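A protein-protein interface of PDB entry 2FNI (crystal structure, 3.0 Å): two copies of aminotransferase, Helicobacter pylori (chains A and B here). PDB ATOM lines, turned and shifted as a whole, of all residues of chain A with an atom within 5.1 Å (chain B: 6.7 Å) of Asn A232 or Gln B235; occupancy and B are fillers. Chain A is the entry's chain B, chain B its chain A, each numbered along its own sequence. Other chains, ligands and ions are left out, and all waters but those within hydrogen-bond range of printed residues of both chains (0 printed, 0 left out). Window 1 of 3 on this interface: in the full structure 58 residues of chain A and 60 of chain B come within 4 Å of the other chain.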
ATOM      1  N   LEU A  28       2.617  -8.079  30.594  1.00  0.00           N
ATOM      2  CA  LEU A  28       4.054  -8.241  30.319  1.00  0.00           C
ATOM      3  C   LEU A  28       4.454  -7.884  28.899  1.00  0.00           C
ATOM      4  O   LEU A  28       5.635  -7.722  28.616  1.00  0.00           O
ATOM      5  CB  LEU A  28       4.514  -9.672  30.601  1.00  0.00           C
ATOM      6  CG  LEU A  28       4.735 -10.105  32.053  1.00  0.00           C
ATOM      7  CD1 LEU A  28       5.237 -11.525  32.104  1.00  0.00           C
ATOM      8  CD2 LEU A  28       5.713  -9.191  32.754  1.00  0.00           C
ATOM      9  N   THR A  29       3.475  -7.774  28.008  1.00  0.00           N
ATOM     10  CA  THR A  29       3.734  -7.445  26.599  1.00  0.00           C
ATOM     11  C   THR A  29       2.503  -6.801  25.954  1.00  0.00           C
ATOM     12  O   THR A  29       1.394  -6.934  26.471  1.00  0.00           O
ATOM     13  CB  THR A  29       4.178  -8.696  25.774  1.00  0.00           C
ATOM     14  OG1 THR A  29       4.744  -8.279  24.526  1.00  0.00           O
ATOM     15  CG2 THR A  29       3.007  -9.617  25.503  1.00  0.00           C
ATOM     16  N   ARG A 230       7.802  -7.508  18.294  1.00  0.00           N
ATOM     17  CA  ARG A 230       7.390  -6.606  19.365  1.00  0.00           C
ATOM     18  C   ARG A 230       8.435  -6.527  20.467  1.00  0.00           C
ATOM     19  O   ARG A 230       9.120  -7.512  20.736  1.00  0.00           O
ATOM     20  CB  ARG A 230       6.066  -7.077  19.977  1.00  0.00           C
ATOM     21  CG  ARG A 230       4.884  -7.110  19.007  1.00  0.00           C
ATOM     22  CD  ARG A 230       3.569  -7.327  19.743  1.00  0.00           C
ATOM     23  NE  ARG A 230       3.529  -8.611  20.421  1.00  0.00           N
ATOM     24  CZ  ARG A 230       2.893  -9.684  19.957  1.00  0.00           C
ATOM     25  NH1 ARG A 230       2.236  -9.625  18.809  1.00  0.00           N
ATOM     26  NH2 ARG A 230       2.902 -10.822  20.643  1.00  0.00           N
ATOM     27  N   LEU A 231       8.558  -5.349  21.085  1.00  0.00           N
ATOM     28  CA  LEU A 231       9.355  -5.172  22.299  1.00  0.00           C
ATOM     29  C   LEU A 231       8.402  -5.370  23.485  1.00  0.00           C
ATOM     30  O   LEU A 231       7.329  -4.790  23.516  1.00  0.00           O
ATOM     31  CB  LEU A 231       9.974  -3.770  22.335  1.00  0.00           C
ATOM     32  CG  LEU A 231      11.099  -3.495  23.343  1.00  0.00           C
ATOM     33  CD1 LEU A 231      12.413  -4.055  22.860  1.00  0.00           C
ATOM     34  CD2 LEU A 231      11.247  -2.011  23.627  1.00  0.00           C
ATOM     35  N   ASN A 232       8.770  -6.202  24.447  1.00  0.00           N
ATOM     36  CA  ASN A 232       7.864  -6.486  25.556  1.00  0.00           C
ATOM     37  C   ASN A 232       7.844  -5.374  26.623  1.00  0.00           C
ATOM     38  O   ASN A 232       8.612  -4.416  26.541  1.00  0.00           O
ATOM     39  CB  ASN A 232       8.217  -7.832  26.171  1.00  0.00           C
ATOM     40  CG  ASN A 232       9.598  -7.842  26.783  1.00  0.00           C
ATOM     41  OD1 ASN A 232      10.476  -8.585  26.351  1.00  0.00           O
ATOM     42  ND2 ASN A 232       9.802  -7.005  27.789  1.00  0.00           N
ATOM     43  N   GLU A 233       6.979  -5.497  27.626  1.00  0.00           N
ATOM     44  CA  GLU A 233       6.823  -4.420  28.602  1.00  0.00           C
ATOM     45  C   GLU A 233       8.027  -4.248  29.508  1.00  0.00           C
ATOM     46  O   GLU A 233       8.329  -3.139  29.929  1.00  0.00           O
ATOM     47  CB  GLU A 233       5.564  -4.612  29.441  1.00  0.00           C
ATOM     48  CG  GLU A 233       4.299  -4.373  28.668  1.00  0.00           C
ATOM     49  CD  GLU A 233       4.149  -2.927  28.224  1.00  0.00           C
ATOM     50  OE1 GLU A 233       4.496  -2.618  27.054  1.00  0.00           O
ATOM     51  OE2 GLU A 233       3.679  -2.102  29.045  1.00  0.00           O
ATOM     52  N   ILE A 234       8.707  -5.344  29.811  1.00  0.00           N
ATOM     53  CA  ILE A 234       9.882  -5.314  30.665  1.00  0.00           C
ATOM     54  C   ILE A 234      10.971  -4.473  30.018  1.00  0.00           C
ATOM     55  O   ILE A 234      11.587  -3.628  30.656  1.00  0.00           O
ATOM     56  CB  ILE A 234      10.439  -6.726  30.877  1.00  0.00           C
ATOM     57  CG1 ILE A 234       9.391  -7.633  31.521  1.00  0.00           C
ATOM     58  CG2 ILE A 234      11.702  -6.687  31.710  1.00  0.00           C
ATOM     59  CD1 ILE A 234       9.790  -9.088  31.513  1.00  0.00           C
ATOM     60  N   GLN A 235      11.208  -4.710  28.735  1.00  0.00           N
ATOM     61  CA  GLN A 235      12.268  -4.011  28.020  1.00  0.00           C
ATOM     62  C   GLN A 235      11.893  -2.563  27.751  1.00  0.00           C
ATOM     63  O   GLN A 235      12.747  -1.667  27.751  1.00  0.00           O
ATOM     64  CB  GLN A 235      12.574  -4.723  26.711  1.00  0.00           C
ATOM     65  CG  GLN A 235      12.976  -6.173  26.906  1.00  0.00           C
ATOM     66  CD  GLN A 235      13.215  -6.883  25.592  1.00  0.00           C
ATOM     67  OE1 GLN A 235      14.308  -7.387  25.347  1.00  0.00           O
ATOM     68  NE2 GLN A 235      12.197  -6.906  24.725  1.00  0.00           N
ATOM     69  N   SER A 236      10.607  -2.338  27.523  1.00  0.00           N
ATOM     70  CA  SER A 236      10.113  -0.998  27.293  1.00  0.00           C
ATOM     71  C   SER A 236      10.315  -0.140  28.533  1.00  0.00           C
ATOM     72  O   SER A 236      10.726   1.018  28.433  1.00  0.00           O
ATOM     73  CB  SER A 236       8.642  -1.048  26.902  1.00  0.00           C
ATOM     74  OG  SER A 236       8.467  -1.902  25.785  1.00  0.00           O
ATOM     75  N   ALA A 237      10.028  -0.709  29.702  1.00  0.00           N
ATOM     76  CA  ALA A 237      10.221   0.010  30.958  1.00  0.00           C
ATOM     77  C   ALA A 237      11.689   0.405  31.120  1.00  0.00           C
ATOM     78  O   ALA A 237      12.013   1.542  31.504  1.00  0.00           O
ATOM     79  CB  ALA A 237       9.767  -0.836  32.117  1.00  0.00           C
ATOM     80  N   VAL B  19      15.338 -12.304  37.637  1.00  0.00           N
ATOM     81  CA  VAL B  19      15.517 -11.184  36.730  1.00  0.00           C
ATOM     82  C   VAL B  19      16.448 -10.112  37.326  1.00  0.00           C
ATOM     83  O   VAL B  19      17.276  -9.549  36.612  1.00  0.00           O
ATOM     84  CB  VAL B  19      14.152 -10.597  36.296  1.00  0.00           C
ATOM     85  CG1 VAL B  19      14.319  -9.268  35.593  1.00  0.00           C
ATOM     86  CG2 VAL B  19      13.431 -11.574  35.395  1.00  0.00           C
ATOM     87  N   VAL B  22      20.255 -10.557  36.967  1.00  0.00           N
ATOM     88  CA  VAL B  22      20.696 -10.321  35.605  1.00  0.00           C
ATOM     89  C   VAL B  22      20.926  -8.837  35.368  1.00  0.00           C
ATOM     90  O   VAL B  22      21.887  -8.455  34.709  1.00  0.00           O
ATOM     91  CB  VAL B  22      19.708 -10.872  34.585  1.00  0.00           C
ATOM     92  CG1 VAL B  22      20.213 -10.639  33.161  1.00  0.00           C
ATOM     93  CG2 VAL B  22      19.511 -12.346  34.829  1.00  0.00           C
ATOM     94  N   LEU B  28      24.039  -8.567  29.413  1.00  0.00           N
ATOM     95  CA  LEU B  28      22.590  -8.463  29.287  1.00  0.00           C
ATOM     96  C   LEU B  28      22.026  -9.294  28.143  1.00  0.00           C
ATOM     97  O   LEU B  28      20.825  -9.572  28.103  1.00  0.00           O
ATOM     98  CB  LEU B  28      22.155  -7.008  29.131  1.00  0.00           C
ATOM     99  CG  LEU B  28      22.088  -6.144  30.386  1.00  0.00           C
ATOM    100  CD1 LEU B  28      21.534  -4.796  30.032  1.00  0.00           C
ATOM    101  CD2 LEU B  28      21.215  -6.789  31.418  1.00  0.00           C
ATOM    102  N   PHE B  37      19.239 -21.917  29.641  1.00  0.00           N
ATOM    103  CA  PHE B  37      17.822 -22.108  29.353  1.00  0.00           C
ATOM    104  C   PHE B  37      17.656 -23.158  28.247  1.00  0.00           C
ATOM    105  O   PHE B  37      16.760 -23.995  28.299  1.00  0.00           O
ATOM    106  CB  PHE B  37      17.176 -20.775  28.961  1.00  0.00           C
ATOM    107  CG  PHE B  37      15.674 -20.839  28.774  1.00  0.00           C
ATOM    108  CD1 PHE B  37      14.898 -21.721  29.507  1.00  0.00           C
ATOM    109  CD2 PHE B  37      15.033 -19.971  27.885  1.00  0.00           C
ATOM    110  CE1 PHE B  37      13.514 -21.758  29.329  1.00  0.00           C
ATOM    111  CE2 PHE B  37      13.660 -20.000  27.716  1.00  0.00           C
ATOM    112  CZ  PHE B  37      12.901 -20.889  28.435  1.00  0.00           C
ATOM    113  N   PHE B  53      14.339 -17.965  20.951  1.00  0.00           N
ATOM    114  CA  PHE B  53      14.154 -16.803  20.086  1.00  0.00           C
ATOM    115  C   PHE B  53      13.355 -15.688  20.780  1.00  0.00           C
ATOM    116  O   PHE B  53      12.764 -15.892  21.847  1.00  0.00           O
ATOM    117  CB  PHE B  53      13.443 -17.209  18.788  1.00  0.00           C
ATOM    118  CG  PHE B  53      14.215 -18.192  17.939  1.00  0.00           C
ATOM    119  CD1 PHE B  53      14.953 -17.763  16.846  1.00  0.00           C
ATOM    120  CD2 PHE B  53      14.179 -19.544  18.215  1.00  0.00           C
ATOM    121  CE1 PHE B  53      15.652 -18.660  16.069  1.00  0.00           C
ATOM    122  CE2 PHE B  53      14.881 -20.442  17.432  1.00  0.00           C
ATOM    123  CZ  PHE B  53      15.619 -19.995  16.366  1.00  0.00           C
ATOM    124  N   ASN B  54      13.335 -14.512  20.162  1.00  0.00           N
ATOM    125  CA  ASN B  54      12.594 -13.391  20.702  1.00  0.00           C
ATOM    126  C   ASN B  54      11.098 -13.664  20.733  1.00  0.00           C
ATOM    127  O   ASN B  54      10.372 -13.086  21.548  1.00  0.00           O
ATOM    128  CB  ASN B  54      12.860 -12.139  19.880  1.00  0.00           C
ATOM    129  CG  ASN B  54      12.208 -12.195  18.504  1.00  0.00           C
ATOM    130  OD1 ASN B  54      11.194 -11.541  18.248  1.00  0.00           O
ATOM    131  ND2 ASN B  54      12.780 -12.986  17.619  1.00  0.00           N
ATOM    132  N   THR B 186       6.358 -18.323  30.556  1.00  0.00           N
ATOM    133  CA  THR B 186       6.602 -17.110  29.787  1.00  0.00           C
ATOM    134  C   THR B 186       7.993 -16.496  29.950  1.00  0.00           C
ATOM    135  O   THR B 186       8.642 -16.626  30.994  1.00  0.00           O
ATOM    136  CB  THR B 186       5.558 -16.028  30.116  1.00  0.00           C
ATOM    137  OG1 THR B 186       5.594 -15.002  29.118  1.00  0.00           O
ATOM    138  CG2 THR B 186       5.851 -15.407  31.464  1.00  0.00           C
ATOM    139  N   THR B 187       8.439 -15.825  28.893  1.00  0.00           N
ATOM    140  CA  THR B 187       9.606 -14.954  28.952  1.00  0.00           C
ATOM    141  C   THR B 187       9.196 -13.568  28.453  1.00  0.00           C
ATOM    142  O   THR B 187      10.007 -12.867  27.844  1.00  0.00           O
ATOM    143  CB  THR B 187      10.783 -15.498  28.099  1.00  0.00           C
ATOM    144  OG1 THR B 187      10.368 -15.668  26.738  1.00  0.00           O
ATOM    145  CG2 THR B 187      11.236 -16.827  28.614  1.00  0.00           C
ATOM    146  N   ALA B 188       7.936 -13.197  28.715  1.00  0.00           N
ATOM    147  CA  ALA B 188       7.296 -11.964  28.193  1.00  0.00           C
ATOM    148  C   ALA B 188       6.990 -12.048  26.682  1.00  0.00           C
ATOM    149  O   ALA B 188       5.833 -12.035  26.248  1.00  0.00           O
ATOM    150  CB  ALA B 188       8.135 -10.746  28.505  1.00  0.00           C
ATOM    151  N   GLU B 189       8.053 -12.091  25.893  1.00  0.00           N
ATOM    152  CA  GLU B 189       7.994 -12.551  24.517  1.00  0.00           C
ATOM    153  C   GLU B 189       9.104 -13.590  24.440  1.00  0.00           C
ATOM    154  O   GLU B 189      10.147 -13.425  25.084  1.00  0.00           O
ATOM    155  CB  GLU B 189       8.274 -11.401  23.538  1.00  0.00           C
ATOM    156  CG  GLU B 189       7.212 -10.311  23.504  1.00  0.00           C
ATOM    157  CD  GLU B 189       6.012 -10.692  22.646  1.00  0.00           C
ATOM    158  OE1 GLU B 189       6.027 -11.787  22.050  1.00  0.00           O
ATOM    159  OE2 GLU B 189       5.052  -9.899  22.565  1.00  0.00           O
ATOM    160  N   GLY B 190       8.882 -14.669  23.696  1.00  0.00           N
ATOM    161  CA  GLY B 190       9.879 -15.727  23.602  1.00  0.00           C
ATOM    162  C   GLY B 190       9.392 -16.907  22.801  1.00  0.00           C
ATOM    163  O   GLY B 190       8.193 -17.089  22.634  1.00  0.00           O
ATOM    164  N   ARG B 230      17.537 -13.100  18.727  1.00  0.00           N
ATOM    165  CA  ARG B 230      18.071 -13.623  19.978  1.00  0.00           C
ATOM    166  C   ARG B 230      17.156 -13.299  21.165  1.00  0.00           C
ATOM    167  O   ARG B 230      16.500 -12.262  21.185  1.00  0.00           O
ATOM    168  CB  ARG B 230      19.465 -13.058  20.248  1.00  0.00           C
ATOM    169  CG  ARG B 230      20.537 -13.420  19.232  1.00  0.00           C
ATOM    170  CD  ARG B 230      21.927 -12.927  19.697  1.00  0.00           C
ATOM    171  NE  ARG B 230      21.981 -11.475  19.878  1.00  0.00           N
ATOM    172  CZ  ARG B 230      22.541 -10.624  19.021  1.00  0.00           C
ATOM    173  NH1 ARG B 230      23.122 -11.074  17.921  1.00  0.00           N
ATOM    174  NH2 ARG B 230      22.530  -9.321  19.264  1.00  0.00           N
ATOM    175  N   LEU B 231      17.113 -14.203  22.142  1.00  0.00           N
ATOM    176  CA  LEU B 231      16.449 -13.952  23.406  1.00  0.00           C
ATOM    177  C   LEU B 231      17.525 -13.430  24.339  1.00  0.00           C
ATOM    178  O   LEU B 231      18.584 -14.046  24.455  1.00  0.00           O
ATOM    179  CB  LEU B 231      15.883 -15.257  23.956  1.00  0.00           C
ATOM    180  CG  LEU B 231      14.907 -15.170  25.135  1.00  0.00           C
ATOM    181  CD1 LEU B 231      13.507 -14.827  24.647  1.00  0.00           C
ATOM    182  CD2 LEU B 231      14.883 -16.475  25.906  1.00  0.00           C
ATOM    183  N   ASN B 232      17.271 -12.301  25.000  1.00  0.00           N
ATOM    184  CA  ASN B 232      18.293 -11.670  25.854  1.00  0.00           C
ATOM    185  C   ASN B 232      18.457 -12.360  27.213  1.00  0.00           C
ATOM    186  O   ASN B 232      17.709 -13.276  27.532  1.00  0.00           O
ATOM    187  CB  ASN B 232      17.994 -10.181  26.027  1.00  0.00           C
ATOM    188  CG  ASN B 232      16.691  -9.932  26.752  1.00  0.00           C
ATOM    189  OD1 ASN B 232      15.751  -9.384  26.189  1.00  0.00           O
ATOM    190  ND2 ASN B 232      16.626 -10.341  28.009  1.00  0.00           N
ATOM    191  N   GLU B 233      19.424 -11.924  28.015  1.00  0.00           N
ATOM    192  CA  GLU B 233      19.696 -12.597  29.283  1.00  0.00           C
ATOM    193  C   GLU B 233      18.597 -12.407  30.324  1.00  0.00           C
ATOM    194  O   GLU B 233      18.342 -13.300  31.128  1.00  0.00           O
ATOM    195  CB  GLU B 233      21.044 -12.170  29.863  1.00  0.00           C
ATOM    196  CG  GLU B 233      22.237 -12.697  29.096  1.00  0.00           C
ATOM    197  CD  GLU B 233      22.372 -14.207  29.177  1.00  0.00           C
ATOM    198  OE1 GLU B 233      21.880 -14.914  28.266  1.00  0.00           O
ATOM    199  OE2 GLU B 233      22.974 -14.687  30.156  1.00  0.00           O
ATOM    200  N   ILE B 234      17.951 -11.246  30.319  1.00  0.00           N
ATOM    201  CA  ILE B 234      16.861 -10.990  31.245  1.00  0.00           C
ATOM    202  C   ILE B 234      15.731 -12.004  31.052  1.00  0.00           C
ATOM    203  O   ILE B 234      15.250 -12.608  32.016  1.00  0.00           O
ATOM    204  CB  ILE B 234      16.288  -9.603  31.040  1.00  0.00           C
ATOM    205  CG1 ILE B 234      17.382  -8.550  31.196  1.00  0.00           C
ATOM    206  CG2 ILE B 234      15.164  -9.362  32.017  1.00  0.00           C
ATOM    207  CD1 ILE B 234      16.960  -7.170  30.774  1.00  0.00           C
ATOM    208  N   GLN B 235      15.313 -12.194  29.802  1.00  0.00           N
ATOM    209  CA  GLN B 235      14.224 -13.104  29.482  1.00  0.00           C
ATOM    210  C   GLN B 235      14.624 -14.559  29.658  1.00  0.00           C
ATOM    211  O   GLN B 235      13.800 -15.391  30.021  1.00  0.00           O
ATOM    212  CB  GLN B 235      13.746 -12.870  28.060  1.00  0.00           C
ATOM    213  CG  GLN B 235      13.338 -11.455  27.802  1.00  0.00           C
ATOM    214  CD  GLN B 235      12.950 -11.248  26.367  1.00  0.00           C
ATOM    215  OE1 GLN B 235      11.834 -10.827  26.072  1.00  0.00           O
ATOM    216  NE2 GLN B 235      13.866 -11.567  25.453  1.00  0.00           N
ATOM    217  N   SER B 236      15.885 -14.875  29.391  1.00  0.00           N
ATOM    218  CA  SER B 236      16.364 -16.239  29.576  1.00  0.00           C
ATOM    219  C   SER B 236      16.349 -16.642  31.046  1.00  0.00           C
ATOM    220  O   SER B 236      15.995 -17.765  31.388  1.00  0.00           O
ATOM    221  CB  SER B 236      17.767 -16.391  29.022  1.00  0.00           C
ATOM    222  OG  SER B 236      17.799 -15.963  27.682  1.00  0.00           O
ATOM    223  N   ALA B 237      16.736 -15.725  31.920  1.00  0.00           N
ATOM    224  CA  ALA B 237      16.677 -16.003  33.346  1.00  0.00           C
ATOM    225  C   ALA B 237      15.235 -16.248  33.759  1.00  0.00           C
ATOM    226  O   ALA B 237      14.949 -17.156  34.522  1.00  0.00           O
ATOM    227  CB  ALA B 237      17.269 -14.863  34.136  1.00  0.00           C
ATOM    228  N   LEU B 238      14.328 -15.436  33.241  1.00  0.00           N
ATOM    229  CA  LEU B 238      12.920 -15.603  33.537  1.00  0.00           C
ATOM    230  C   LEU B 238      12.469 -16.970  33.066  1.00  0.00           C
ATOM    231  O   LEU B 238      11.784 -17.683  33.790  1.00  0.00           O
ATOM    232  CB  LEU B 238      12.099 -14.494  32.866  1.00  0.00           C
ATOM    233  CG  LEU B 238      10.591 -14.444  33.116  1.00  0.00           C
ATOM    234  CD1 LEU B 238      10.253 -14.617  34.597  1.00  0.00           C
ATOM    235  CD2 LEU B 238      10.002 -13.151  32.563  1.00  0.00           C
ATOM    236  N   GLY B 239      12.881 -17.339  31.858  1.00  0.00           N
ATOM    237  CA  GLY B 239      12.476 -18.605  31.253  1.00  0.00           C
ATOM    238  C   GLY B 239      12.963 -19.789  32.048  1.00  0.00           C
ATOM    239  O   GLY B 239      12.221 -20.732  32.299  1.00  0.00           O
ATOM    240  N   LEU B 240      14.230 -19.739  32.438  1.00  0.00           N
ATOM    241  CA  LEU B 240      14.815 -20.763  33.284  1.00  0.00           C
ATOM    242  C   LEU B 240      13.988 -20.948  34.536  1.00  0.00           C
ATOM    243  O   LEU B 240      13.611 -22.059  34.889  1.00  0.00           O
ATOM    244  CB  LEU B 240      16.236 -20.374  33.666  1.00  0.00           C
ATOM    245  CG  LEU B 240      17.321 -21.309  33.147  1.00  0.00           C
ATOM    246  CD1 LEU B 240      18.676 -20.748  33.507  1.00  0.00           C
ATOM    247  CD2 LEU B 240      17.129 -22.703  33.750  1.00  0.00           C
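CD1 of Leu A28 touches CG2 of Thr B186, at 3.98 Å. O of Leu A28 touches CB of Ala B188, at 3.9 Å. Thr A29 touches Ala B188 (CB to O, 3.8 Å). Asn A232 touches Ala B188. CB of Asn A232 touches CG of Glu B189, 3.8 Å away. CD1 of Ile A234 touches CB of Ala B188, 3.8 Å away.
Printed residues of chain A that touch a printed residue of chain B: Leu A28, Thr A29, Arg A230, Asn A232, Ile A234 and Gln A235. Hydrophobic or aromatic side chains of chain A within 4 Å of the printed part of chain B: Leu A28 and Ile A234. Hydrophobic or aromatic side chains of chain B that line the printed part of chain A: Ala B188. Among the printed residues, Asp or Glu carboxylates within 4 Å of a Lys or Arg side-chain nitrogen of the other chain: Arg A230 with Glu B189 (2.9 Å).
The side-chain amide nitrogen of Asn A232 lies close to the backbone NH of Gln A235 (2.9 Å). OG of Ser A236 lies within hydrogen-bond range of O of Asn A232 (2.6 Å). O of Leu A28 is in hydrogen-bond range of N of Glu A233. O of Asn B232 sits at hydrogen-bond distance from OG of Ser B236, 2.7 Å away. N of Ala B188 sits at hydrogen-bond distance from OG1 of Thr B186 (3.0 Å). The side-chain amide nitrogen of Asn B232 sits close to the backbone NH of Gln B235 (2.9 Å).
Of the printed residues of chain B, Leu A28 touches Thr B186 (3.98 Å) and Ala B188 (3.9 Å). Of the printed residues of chain B, Ile A234 touches Ala B188. Of the printed residues of chain A, Thr B186 touches Leu A28. Printed residues of chain A within 4 Å of Ala B188: Leu A28 (3.9 Å), Thr A29 (3.8 Å), Asn A232 (3.7 Å) and Ile A234 (3.8 Å). Of the printed residues of chain A, Glu B189 touches Thr A29 (2.6 Å), Arg A230 (2.9 Å) and Asn A232 (3.8 Å). Arg B230 touches none of the printed residues of chain A. Gln B235 touches just one residue of chain A: Asn A232 (2.6 Å).
The guanidinium group (NE) of Arg A230 lies within salt-bridge range of the side-chain carboxylate (OE2) of Glu B189 (2.9 Å). The side-chain amide oxygen of Gln B235 lies close to the side-chain amide oxygen of Asn A232 (2.6 Å). The side-chain hydroxyl of Thr A29 sits at hydrogen-bond distance from the side-chain carboxylate of Glu B189 (2.6 Å). The side-chain amide oxygen (OE1) of Gln A235 lies close to the side-chain amide oxygen (OD1) of Asn B232 (2.6 Å).
Asn A232 touches Gln B235, and with the chains exchanged Gln A235 touches Asn B232. Positions printed for both chains: 28, 230, 231, 232, 233, 234, 235, 236 and 237. Of the 10 pairs that touch across the chains among the printed residues, 2 have their exchanged pair printed and touching as well.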
